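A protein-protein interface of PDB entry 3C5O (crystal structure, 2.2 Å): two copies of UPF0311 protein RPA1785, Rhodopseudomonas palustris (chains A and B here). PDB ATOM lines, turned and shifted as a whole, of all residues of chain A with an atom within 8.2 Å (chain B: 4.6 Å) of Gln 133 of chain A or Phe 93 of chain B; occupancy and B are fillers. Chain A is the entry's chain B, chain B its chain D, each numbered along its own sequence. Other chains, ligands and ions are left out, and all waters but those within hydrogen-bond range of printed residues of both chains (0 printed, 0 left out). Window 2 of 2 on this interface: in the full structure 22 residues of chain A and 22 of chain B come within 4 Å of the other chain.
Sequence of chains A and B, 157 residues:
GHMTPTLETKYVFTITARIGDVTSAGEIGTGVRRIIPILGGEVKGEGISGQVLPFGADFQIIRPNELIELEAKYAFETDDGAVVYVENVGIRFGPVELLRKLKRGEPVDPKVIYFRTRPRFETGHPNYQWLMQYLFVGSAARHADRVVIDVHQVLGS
Printed residues of chain B within 4 Å of Met 132 of chain A: Leu 67 (3.8 Å). Of the printed residues of chain B, Gln 133 of chain A touches Ile 91, Phe 93 and Tyr 114. Arg 92 of chain B touches none of the printed residues of chain A. Phe 93 of chain B touches just one residue of chain A: Gln 133 (3.6 Å). Gly 94 of chain B touches none of the printed residues of chain A. Printed residues of chain A within 4 Å of Tyr 114 of chain B: Gln 133, Tyr 134, Leu 135 and Val 154.
Met 132 of chain A touches Leu 67 of chain B. CD1 of Ile 91 of chain B touches O of Gln 133 of chain A, at 3.4 Å. Phe 93 of chain B touches Gln 133 of chain A (CE1 to CD, 3.6 Å). Tyr 114 of chain B touches Gln 133 of chain A (CE2 to O, 3.7 Å). Tyr 134 of chain A touches Ile 91 of chain B (N to CD1, 3.6 Å). CA of Tyr 134 of chain A touches OH of Tyr 114 of chain B, 3.5 Å away.
Hydrophobic or aromatic side chains of chain A within 4 Å of the printed part of chain B: Tyr 134, Leu 135 and Val 154. Printed residues of chain B that touch a printed residue of chain A: Leu 67, Ile 91, Phe 93 and Tyr 114. Along chain B the printed residues that touch a printed residue of chain A span positions 67 to 114. Among the printed residues, 8 pairs touch across the chains.
No position is printed for both chains. Of the 8 pairs that touch across the chains among the printed residues, none has its exchanged pair printed and touching as well.
N of Leu 135 of chain A sits at hydrogen-bond distance from OH of Tyr 114 of chain B. OH of Tyr 114 of chain B lies within hydrogen-bond range of O of Val 154 of chain A, at 2.6 Å.
The backbone carbonyl oxygen (O) of Tyr 114 of chain B is in hydrogen-bond range of the backbone NH (N) of Phe 93 of chain B, 2.8 Å away. The backbone carbonyl oxygen (O) of Leu 135 of chain A lies within hydrogen-bond range of the backbone NH (N) of Val 154 of chain A, 2.8 Å away. The backbone NH (N) of Leu 67 of chain B sits at hydrogen-bond distance from the side-chain amide oxygen (OD1) of Asn 65 of chain B, at 3.2 Å.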
ATOM      1  N   PHE A 121      27.388 -14.909  29.395  1.00  0.00           N
ATOM      2  CA  PHE A 121      28.275 -15.152  28.261  1.00  0.00           C
ATOM      3  C   PHE A 121      27.727 -14.584  26.971  1.00  0.00           C
ATOM      4  O   PHE A 121      26.505 -14.552  26.769  1.00  0.00           O
ATOM      5  CB  PHE A 121      28.511 -16.660  28.108  1.00  0.00           C
ATOM      6  CG  PHE A 121      28.961 -17.320  29.379  1.00  0.00           C
ATOM      7  CD1 PHE A 121      30.253 -17.136  29.839  1.00  0.00           C
ATOM      8  CD2 PHE A 121      28.077 -18.100  30.120  1.00  0.00           C
ATOM      9  CE1 PHE A 121      30.670 -17.714  31.039  1.00  0.00           C
ATOM     10  CE2 PHE A 121      28.480 -18.714  31.314  1.00  0.00           C
ATOM     11  CZ  PHE A 121      29.778 -18.512  31.777  1.00  0.00           C
ATOM     12  N   PRO A 126      28.877 -21.207  16.809  1.00  0.00           N
ATOM     13  CA  PRO A 126      27.695 -22.075  16.759  1.00  0.00           C
ATOM     14  C   PRO A 126      27.582 -23.115  17.859  1.00  0.00           C
ATOM     15  O   PRO A 126      26.462 -23.470  18.207  1.00  0.00           O
ATOM     16  CB  PRO A 126      27.822 -22.766  15.388  1.00  0.00           C
ATOM     17  CG  PRO A 126      28.561 -21.810  14.584  1.00  0.00           C
ATOM     18  CD  PRO A 126      29.567 -21.175  15.505  1.00  0.00           C
ATOM     19  N   TYR A 128      28.640 -22.995  20.937  1.00  0.00           N
ATOM     20  CA  TYR A 128      28.560 -22.409  22.275  1.00  0.00           C
ATOM     21  C   TYR A 128      27.412 -21.429  22.402  1.00  0.00           C
ATOM     22  O   TYR A 128      27.323 -20.675  23.361  1.00  0.00           O
ATOM     23  CB  TYR A 128      29.897 -21.753  22.663  1.00  0.00           C
ATOM     24  CG  TYR A 128      31.016 -22.757  22.666  1.00  0.00           C
ATOM     25  CD1 TYR A 128      31.799 -22.965  21.523  1.00  0.00           C
ATOM     26  CD2 TYR A 128      31.245 -23.558  23.770  1.00  0.00           C
ATOM     27  CE1 TYR A 128      32.814 -23.906  21.517  1.00  0.00           C
ATOM     28  CE2 TYR A 128      32.247 -24.511  23.760  1.00  0.00           C
ATOM     29  CZ  TYR A 128      33.032 -24.673  22.639  1.00  0.00           C
ATOM     30  OH  TYR A 128      34.036 -25.623  22.646  1.00  0.00           O
ATOM     31  N   GLN A 129      26.536 -21.473  21.417  1.00  0.00           N
ATOM     32  CA  GLN A 129      25.319 -20.682  21.366  1.00  0.00           C
ATOM     33  C   GLN A 129      24.482 -20.869  22.626  1.00  0.00           C
ATOM     34  O   GLN A 129      23.877 -19.918  23.120  1.00  0.00           O
ATOM     35  CB  GLN A 129      24.510 -21.116  20.126  1.00  0.00           C
ATOM     36  CG  GLN A 129      23.967 -20.009  19.233  1.00  0.00           C
ATOM     37  CD  GLN A 129      25.040 -19.066  18.689  1.00  0.00           C
ATOM     38  OE1 GLN A 129      25.869 -18.568  19.442  1.00  0.00           O
ATOM     39  NE2 GLN A 129      25.004 -18.801  17.353  1.00  0.00           N
ATOM     40  N   TRP A 130      24.459 -22.094  23.145  1.00  0.00           N
ATOM     41  CA  TRP A 130      23.714 -22.402  24.372  1.00  0.00           C
ATOM     42  C   TRP A 130      24.119 -21.526  25.566  1.00  0.00           C
ATOM     43  O   TRP A 130      23.341 -21.370  26.494  1.00  0.00           O
ATOM     44  CB  TRP A 130      23.820 -23.894  24.738  1.00  0.00           C
ATOM     45  CG  TRP A 130      25.229 -24.377  25.094  1.00  0.00           C
ATOM     46  CD1 TRP A 130      26.241 -24.666  24.215  1.00  0.00           C
ATOM     47  CD2 TRP A 130      25.759 -24.632  26.406  1.00  0.00           C
ATOM     48  NE1 TRP A 130      27.360 -25.074  24.900  1.00  0.00           N
ATOM     49  CE2 TRP A 130      27.096 -25.058  26.242  1.00  0.00           C
ATOM     50  CE3 TRP A 130      25.232 -24.555  27.700  1.00  0.00           C
ATOM     51  CZ2 TRP A 130      27.914 -25.400  27.318  1.00  0.00           C
ATOM     52  CZ3 TRP A 130      26.059 -24.892  28.776  1.00  0.00           C
ATOM     53  CH2 TRP A 130      27.379 -25.312  28.574  1.00  0.00           C
ATOM     54  N   LEU A 131      25.336 -20.974  25.543  1.00  0.00           N
ATOM     55  CA  LEU A 131      25.832 -20.148  26.646  1.00  0.00           C
ATOM     56  C   LEU A 131      25.016 -18.856  26.851  1.00  0.00           C
ATOM     57  O   LEU A 131      25.009 -18.285  27.943  1.00  0.00           O
ATOM     58  CB  LEU A 131      27.328 -19.828  26.486  1.00  0.00           C
ATOM     59  CG  LEU A 131      28.307 -21.010  26.605  1.00  0.00           C
ATOM     60  CD1 LEU A 131      29.727 -20.503  26.515  1.00  0.00           C
ATOM     61  CD2 LEU A 131      28.125 -21.776  27.903  1.00  0.00           C
ATOM     62  N   MET A 132      24.294 -18.430  25.819  1.00  0.00           N
ATOM     63  CA  MET A 132      23.458 -17.255  25.935  1.00  0.00           C
ATOM     64  C   MET A 132      21.982 -17.580  25.972  1.00  0.00           C
ATOM     65  O   MET A 132      21.155 -16.667  25.934  1.00  0.00           O
ATOM     66  CB  MET A 132      23.716 -16.310  24.773  1.00  0.00           C
ATOM     67  CG  MET A 132      25.085 -16.470  24.215  1.00  0.00           C
ATOM     68  SD  MET A 132      25.071 -15.895  22.416  1.00  0.00           S
ATOM     69  CE  MET A 132      25.519 -14.063  22.796  1.00  0.00           C
ATOM     70  N   GLN A 133      21.653 -18.861  26.065  1.00  0.00           N
ATOM     71  CA  GLN A 133      20.263 -19.302  26.120  1.00  0.00           C
ATOM     72  C   GLN A 133      19.791 -19.771  27.514  1.00  0.00           C
ATOM     73  O   GLN A 133      18.635 -20.176  27.684  1.00  0.00           O
ATOM     74  CB  GLN A 133      20.035 -20.422  25.099  1.00  0.00           C
ATOM     75  CG  GLN A 133      20.432 -20.078  23.668  1.00  0.00           C
ATOM     76  CD  GLN A 133      20.195 -21.250  22.702  1.00  0.00           C
ATOM     77  OE1 GLN A 133      19.736 -22.334  23.095  1.00  0.00           O
ATOM     78  NE2 GLN A 133      20.512 -21.032  21.438  1.00  0.00           N
ATOM     79  N   TYR A 134      20.686 -19.728  28.495  1.00  0.00           N
ATOM     80  CA  TYR A 134      20.401 -20.155  29.866  1.00  0.00           C
ATOM     81  C   TYR A 134      20.927 -19.109  30.844  1.00  0.00           C
ATOM     82  O   TYR A 134      21.809 -18.332  30.509  1.00  0.00           O
ATOM     83  CB  TYR A 134      21.070 -21.503  30.169  1.00  0.00           C
ATOM     84  CG  TYR A 134      20.535 -22.674  29.363  1.00  0.00           C
ATOM     85  CD1 TYR A 134      19.470 -23.449  29.842  1.00  0.00           C
ATOM     86  CD2 TYR A 134      21.098 -23.017  28.143  1.00  0.00           C
ATOM     87  CE1 TYR A 134      18.977 -24.533  29.116  1.00  0.00           C
ATOM     88  CE2 TYR A 134      20.601 -24.095  27.391  1.00  0.00           C
ATOM     89  CZ  TYR A 134      19.541 -24.849  27.885  1.00  0.00           C
ATOM     90  OH  TYR A 134      19.060 -25.923  27.163  1.00  0.00           O
ATOM     91  N   LEU A 135      20.385 -19.098  32.052  1.00  0.00           N
ATOM     92  CA  LEU A 135      21.011 -18.377  33.145  1.00  0.00           C
ATOM     93  C   LEU A 135      22.025 -19.306  33.797  1.00  0.00           C
ATOM     94  O   LEU A 135      21.840 -20.535  33.807  1.00  0.00           O
ATOM     95  CB  LEU A 135      19.954 -17.997  34.163  1.00  0.00           C
ATOM     96  CG  LEU A 135      20.124 -16.851  35.139  1.00  0.00           C
ATOM     97  CD1 LEU A 135      19.769 -15.595  34.426  1.00  0.00           C
ATOM     98  CD2 LEU A 135      19.170 -17.067  36.295  1.00  0.00           C
ATOM     99  N   PHE A 136      23.085 -18.733  34.358  1.00  0.00           N
ATOM    100  CA  PHE A 136      24.090 -19.531  35.036  1.00  0.00           C
ATOM    101  C   PHE A 136      24.360 -18.925  36.394  1.00  0.00           C
ATOM    102  O   PHE A 136      24.191 -17.712  36.605  1.00  0.00           O
ATOM    103  CB  PHE A 136      25.391 -19.600  34.230  1.00  0.00           C
ATOM    104  CG  PHE A 136      25.245 -20.231  32.873  1.00  0.00           C
ATOM    105  CD1 PHE A 136      25.580 -21.559  32.667  1.00  0.00           C
ATOM    106  CD2 PHE A 136      24.819 -19.478  31.779  1.00  0.00           C
ATOM    107  CE1 PHE A 136      25.442 -22.152  31.402  1.00  0.00           C
ATOM    108  CE2 PHE A 136      24.691 -20.057  30.516  1.00  0.00           C
ATOM    109  CZ  PHE A 136      25.003 -21.400  30.326  1.00  0.00           C
ATOM    110  N   GLN A 153      24.623 -24.443  35.268  1.00  0.00           N
ATOM    111  CA  GLN A 153      23.556 -24.070  34.355  1.00  0.00           C
ATOM    112  C   GLN A 153      22.239 -24.117  35.114  1.00  0.00           C
ATOM    113  O   GLN A 153      21.942 -25.136  35.749  1.00  0.00           O
ATOM    114  CB  GLN A 153      23.518 -25.080  33.216  1.00  0.00           C
ATOM    115  CG  GLN A 153      22.609 -24.715  32.078  1.00  0.00           C
ATOM    116  CD  GLN A 153      22.449 -25.841  31.066  1.00  0.00           C
ATOM    117  OE1 GLN A 153      22.031 -25.616  29.927  1.00  0.00           O
ATOM    118  NE2 GLN A 153      22.752 -27.060  31.483  1.00  0.00           N
ATOM    119  N   VAL A 154      21.455 -23.031  35.068  1.00  0.00           N
ATOM    120  CA  VAL A 154      20.119 -23.046  35.678  1.00  0.00           C
ATOM    121  C   VAL A 154      19.118 -23.656  34.710  1.00  0.00           C
ATOM    122  O   VAL A 154      18.923 -23.174  33.578  1.00  0.00           O
ATOM    123  CB  VAL A 154      19.606 -21.666  36.114  1.00  0.00           C
ATOM    124  CG1 VAL A 154      18.141 -21.765  36.605  1.00  0.00           C
ATOM    125  CG2 VAL A 154      20.502 -21.067  37.203  1.00  0.00           C
ATOM    126  N   ASN B  65      16.093 -13.991  17.176  1.00  0.00           N
ATOM    127  CA  ASN B  65      15.737 -15.392  17.420  1.00  0.00           C
ATOM    128  C   ASN B  65      14.547 -15.570  18.375  1.00  0.00           C
ATOM    129  O   ASN B  65      14.126 -16.698  18.653  1.00  0.00           O
ATOM    130  CB  ASN B  65      16.953 -16.213  17.872  1.00  0.00           C
ATOM    131  CG  ASN B  65      17.351 -15.961  19.329  1.00  0.00           C
ATOM    132  OD1 ASN B  65      16.878 -15.035  19.991  1.00  0.00           O
ATOM    133  ND2 ASN B  65      18.240 -16.801  19.828  1.00  0.00           N
ATOM    134  N   LEU B  67      14.164 -14.789  21.610  1.00  0.00           N
ATOM    135  CA  LEU B  67      14.483 -14.762  23.030  1.00  0.00           C
ATOM    136  C   LEU B  67      14.241 -13.346  23.556  1.00  0.00           C
ATOM    137  O   LEU B  67      14.544 -12.352  22.876  1.00  0.00           O
ATOM    138  CB  LEU B  67      15.938 -15.177  23.258  1.00  0.00           C
ATOM    139  CG  LEU B  67      16.477 -15.238  24.691  1.00  0.00           C
ATOM    140  CD1 LEU B  67      17.596 -16.265  24.786  1.00  0.00           C
ATOM    141  CD2 LEU B  67      16.944 -13.869  25.163  1.00  0.00           C
ATOM    142  N   ILE B  91      15.973 -13.981  31.217  1.00  0.00           N
ATOM    143  CA  ILE B  91      15.650 -14.371  29.843  1.00  0.00           C
ATOM    144  C   ILE B  91      14.395 -15.260  29.757  1.00  0.00           C
ATOM    145  O   ILE B  91      14.062 -15.994  30.696  1.00  0.00           O
ATOM    146  CB  ILE B  91      16.840 -15.037  29.101  1.00  0.00           C
ATOM    147  CG1 ILE B  91      17.301 -16.294  29.824  1.00  0.00           C
ATOM    148  CG2 ILE B  91      18.036 -14.069  28.959  1.00  0.00           C
ATOM    149  CD1 ILE B  91      18.318 -17.082  29.034  1.00  0.00           C
ATOM    150  N   ARG B  92      13.684 -15.147  28.642  1.00  0.00           N
ATOM    151  CA  ARG B  92      12.597 -16.053  28.318  1.00  0.00           C
ATOM    152  C   ARG B  92      12.858 -16.607  26.924  1.00  0.00           C
ATOM    153  O   ARG B  92      13.001 -15.855  25.953  1.00  0.00           O
ATOM    154  CB  ARG B  92      11.240 -15.363  28.415  1.00  0.00           C
ATOM    155  CG  ARG B  92      10.073 -16.280  28.092  1.00  0.00           C
ATOM    156  CD  ARG B  92       8.778 -15.813  28.723  1.00  0.00           C
ATOM    157  NE  ARG B  92       8.189 -14.635  28.071  1.00  0.00           N
ATOM    158  CZ  ARG B  92       8.142 -13.419  28.612  1.00  0.00           C
ATOM    159  NH1 ARG B  92       7.574 -12.418  27.956  1.00  0.00           N
ATOM    160  NH2 ARG B  92       8.656 -13.204  29.813  1.00  0.00           N
ATOM    161  N   PHE B  93      12.965 -17.925  26.841  1.00  0.00           N
ATOM    162  CA  PHE B  93      13.262 -18.602  25.588  1.00  0.00           C
ATOM    163  C   PHE B  93      12.486 -19.916  25.505  1.00  0.00           C
ATOM    164  O   PHE B  93      11.881 -20.341  26.490  1.00  0.00           O
ATOM    165  CB  PHE B  93      14.769 -18.864  25.483  1.00  0.00           C
ATOM    166  CG  PHE B  93      15.244 -19.184  24.079  1.00  0.00           C
ATOM    167  CD1 PHE B  93      16.190 -20.181  23.867  1.00  0.00           C
ATOM    168  CD2 PHE B  93      14.744 -18.487  22.974  1.00  0.00           C
ATOM    169  CE1 PHE B  93      16.636 -20.474  22.575  1.00  0.00           C
ATOM    170  CE2 PHE B  93      15.179 -18.778  21.678  1.00  0.00           C
ATOM    171  CZ  PHE B  93      16.122 -19.772  21.477  1.00  0.00           C
ATOM    172  N   GLY B  94      12.502 -20.538  24.325  1.00  0.00           N
ATOM    173  CA  GLY B  94      11.828 -21.811  24.064  1.00  0.00           C
ATOM    174  C   GLY B  94      11.699 -22.033  22.569  1.00  0.00           C
ATOM    175  O   GLY B  94      12.168 -21.208  21.772  1.00  0.00           O
ATOM    176  N   LEU B  99       6.731 -19.372  21.902  1.00  0.00           N
ATOM    177  CA  LEU B  99       7.025 -17.966  22.204  1.00  0.00           C
ATOM    178  C   LEU B  99       6.072 -17.023  21.470  1.00  0.00           C
ATOM    179  O   LEU B  99       5.625 -16.019  22.037  1.00  0.00           O
ATOM    180  CB  LEU B  99       8.483 -17.598  21.863  1.00  0.00           C
ATOM    181  CG  LEU B  99       9.654 -18.434  22.393  1.00  0.00           C
ATOM    182  CD1 LEU B  99      10.967 -17.981  21.762  1.00  0.00           C
ATOM    183  CD2 LEU B  99       9.733 -18.392  23.918  1.00  0.00           C
ATOM    184  N   ILE B 113       8.455 -23.769  28.939  1.00  0.00           N
ATOM    185  CA  ILE B 113       9.141 -22.556  28.520  1.00  0.00           C
ATOM    186  C   ILE B 113      10.203 -22.193  29.547  1.00  0.00           C
ATOM    187  O   ILE B 113       9.962 -22.292  30.754  1.00  0.00           O
ATOM    188  CB  ILE B 113       8.142 -21.399  28.366  1.00  0.00           C
ATOM    189  CG1 ILE B 113       7.317 -21.599  27.101  1.00  0.00           C
ATOM    190  CG2 ILE B 113       8.841 -20.046  28.313  1.00  0.00           C
ATOM    191  CD1 ILE B 113       6.087 -20.779  27.102  1.00  0.00           C
ATOM    192  N   TYR B 114      11.370 -21.772  29.057  1.00  0.00           N
ATOM    193  CA  TYR B 114      12.487 -21.383  29.915  1.00  0.00           C
ATOM    194  C   TYR B 114      12.440 -19.893  30.269  1.00  0.00           C
ATOM    195  O   TYR B 114      12.652 -19.028  29.422  1.00  0.00           O
ATOM    196  CB  TYR B 114      13.818 -21.720  29.249  1.00  0.00           C
ATOM    197  CG  TYR B 114      15.021 -21.487  30.130  1.00  0.00           C
ATOM    198  CD1 TYR B 114      15.465 -22.481  31.005  1.00  0.00           C
ATOM    199  CD2 TYR B 114      15.722 -20.286  30.083  1.00  0.00           C
ATOM    200  CE1 TYR B 114      16.578 -22.282  31.809  1.00  0.00           C
ATOM    201  CE2 TYR B 114      16.839 -20.073  30.897  1.00  0.00           C
ATOM    202  CZ  TYR B 114      17.254 -21.076  31.754  1.00  0.00           C
ATOM    203  OH  TYR B 114      18.348 -20.885  32.561  1.00  0.00           O
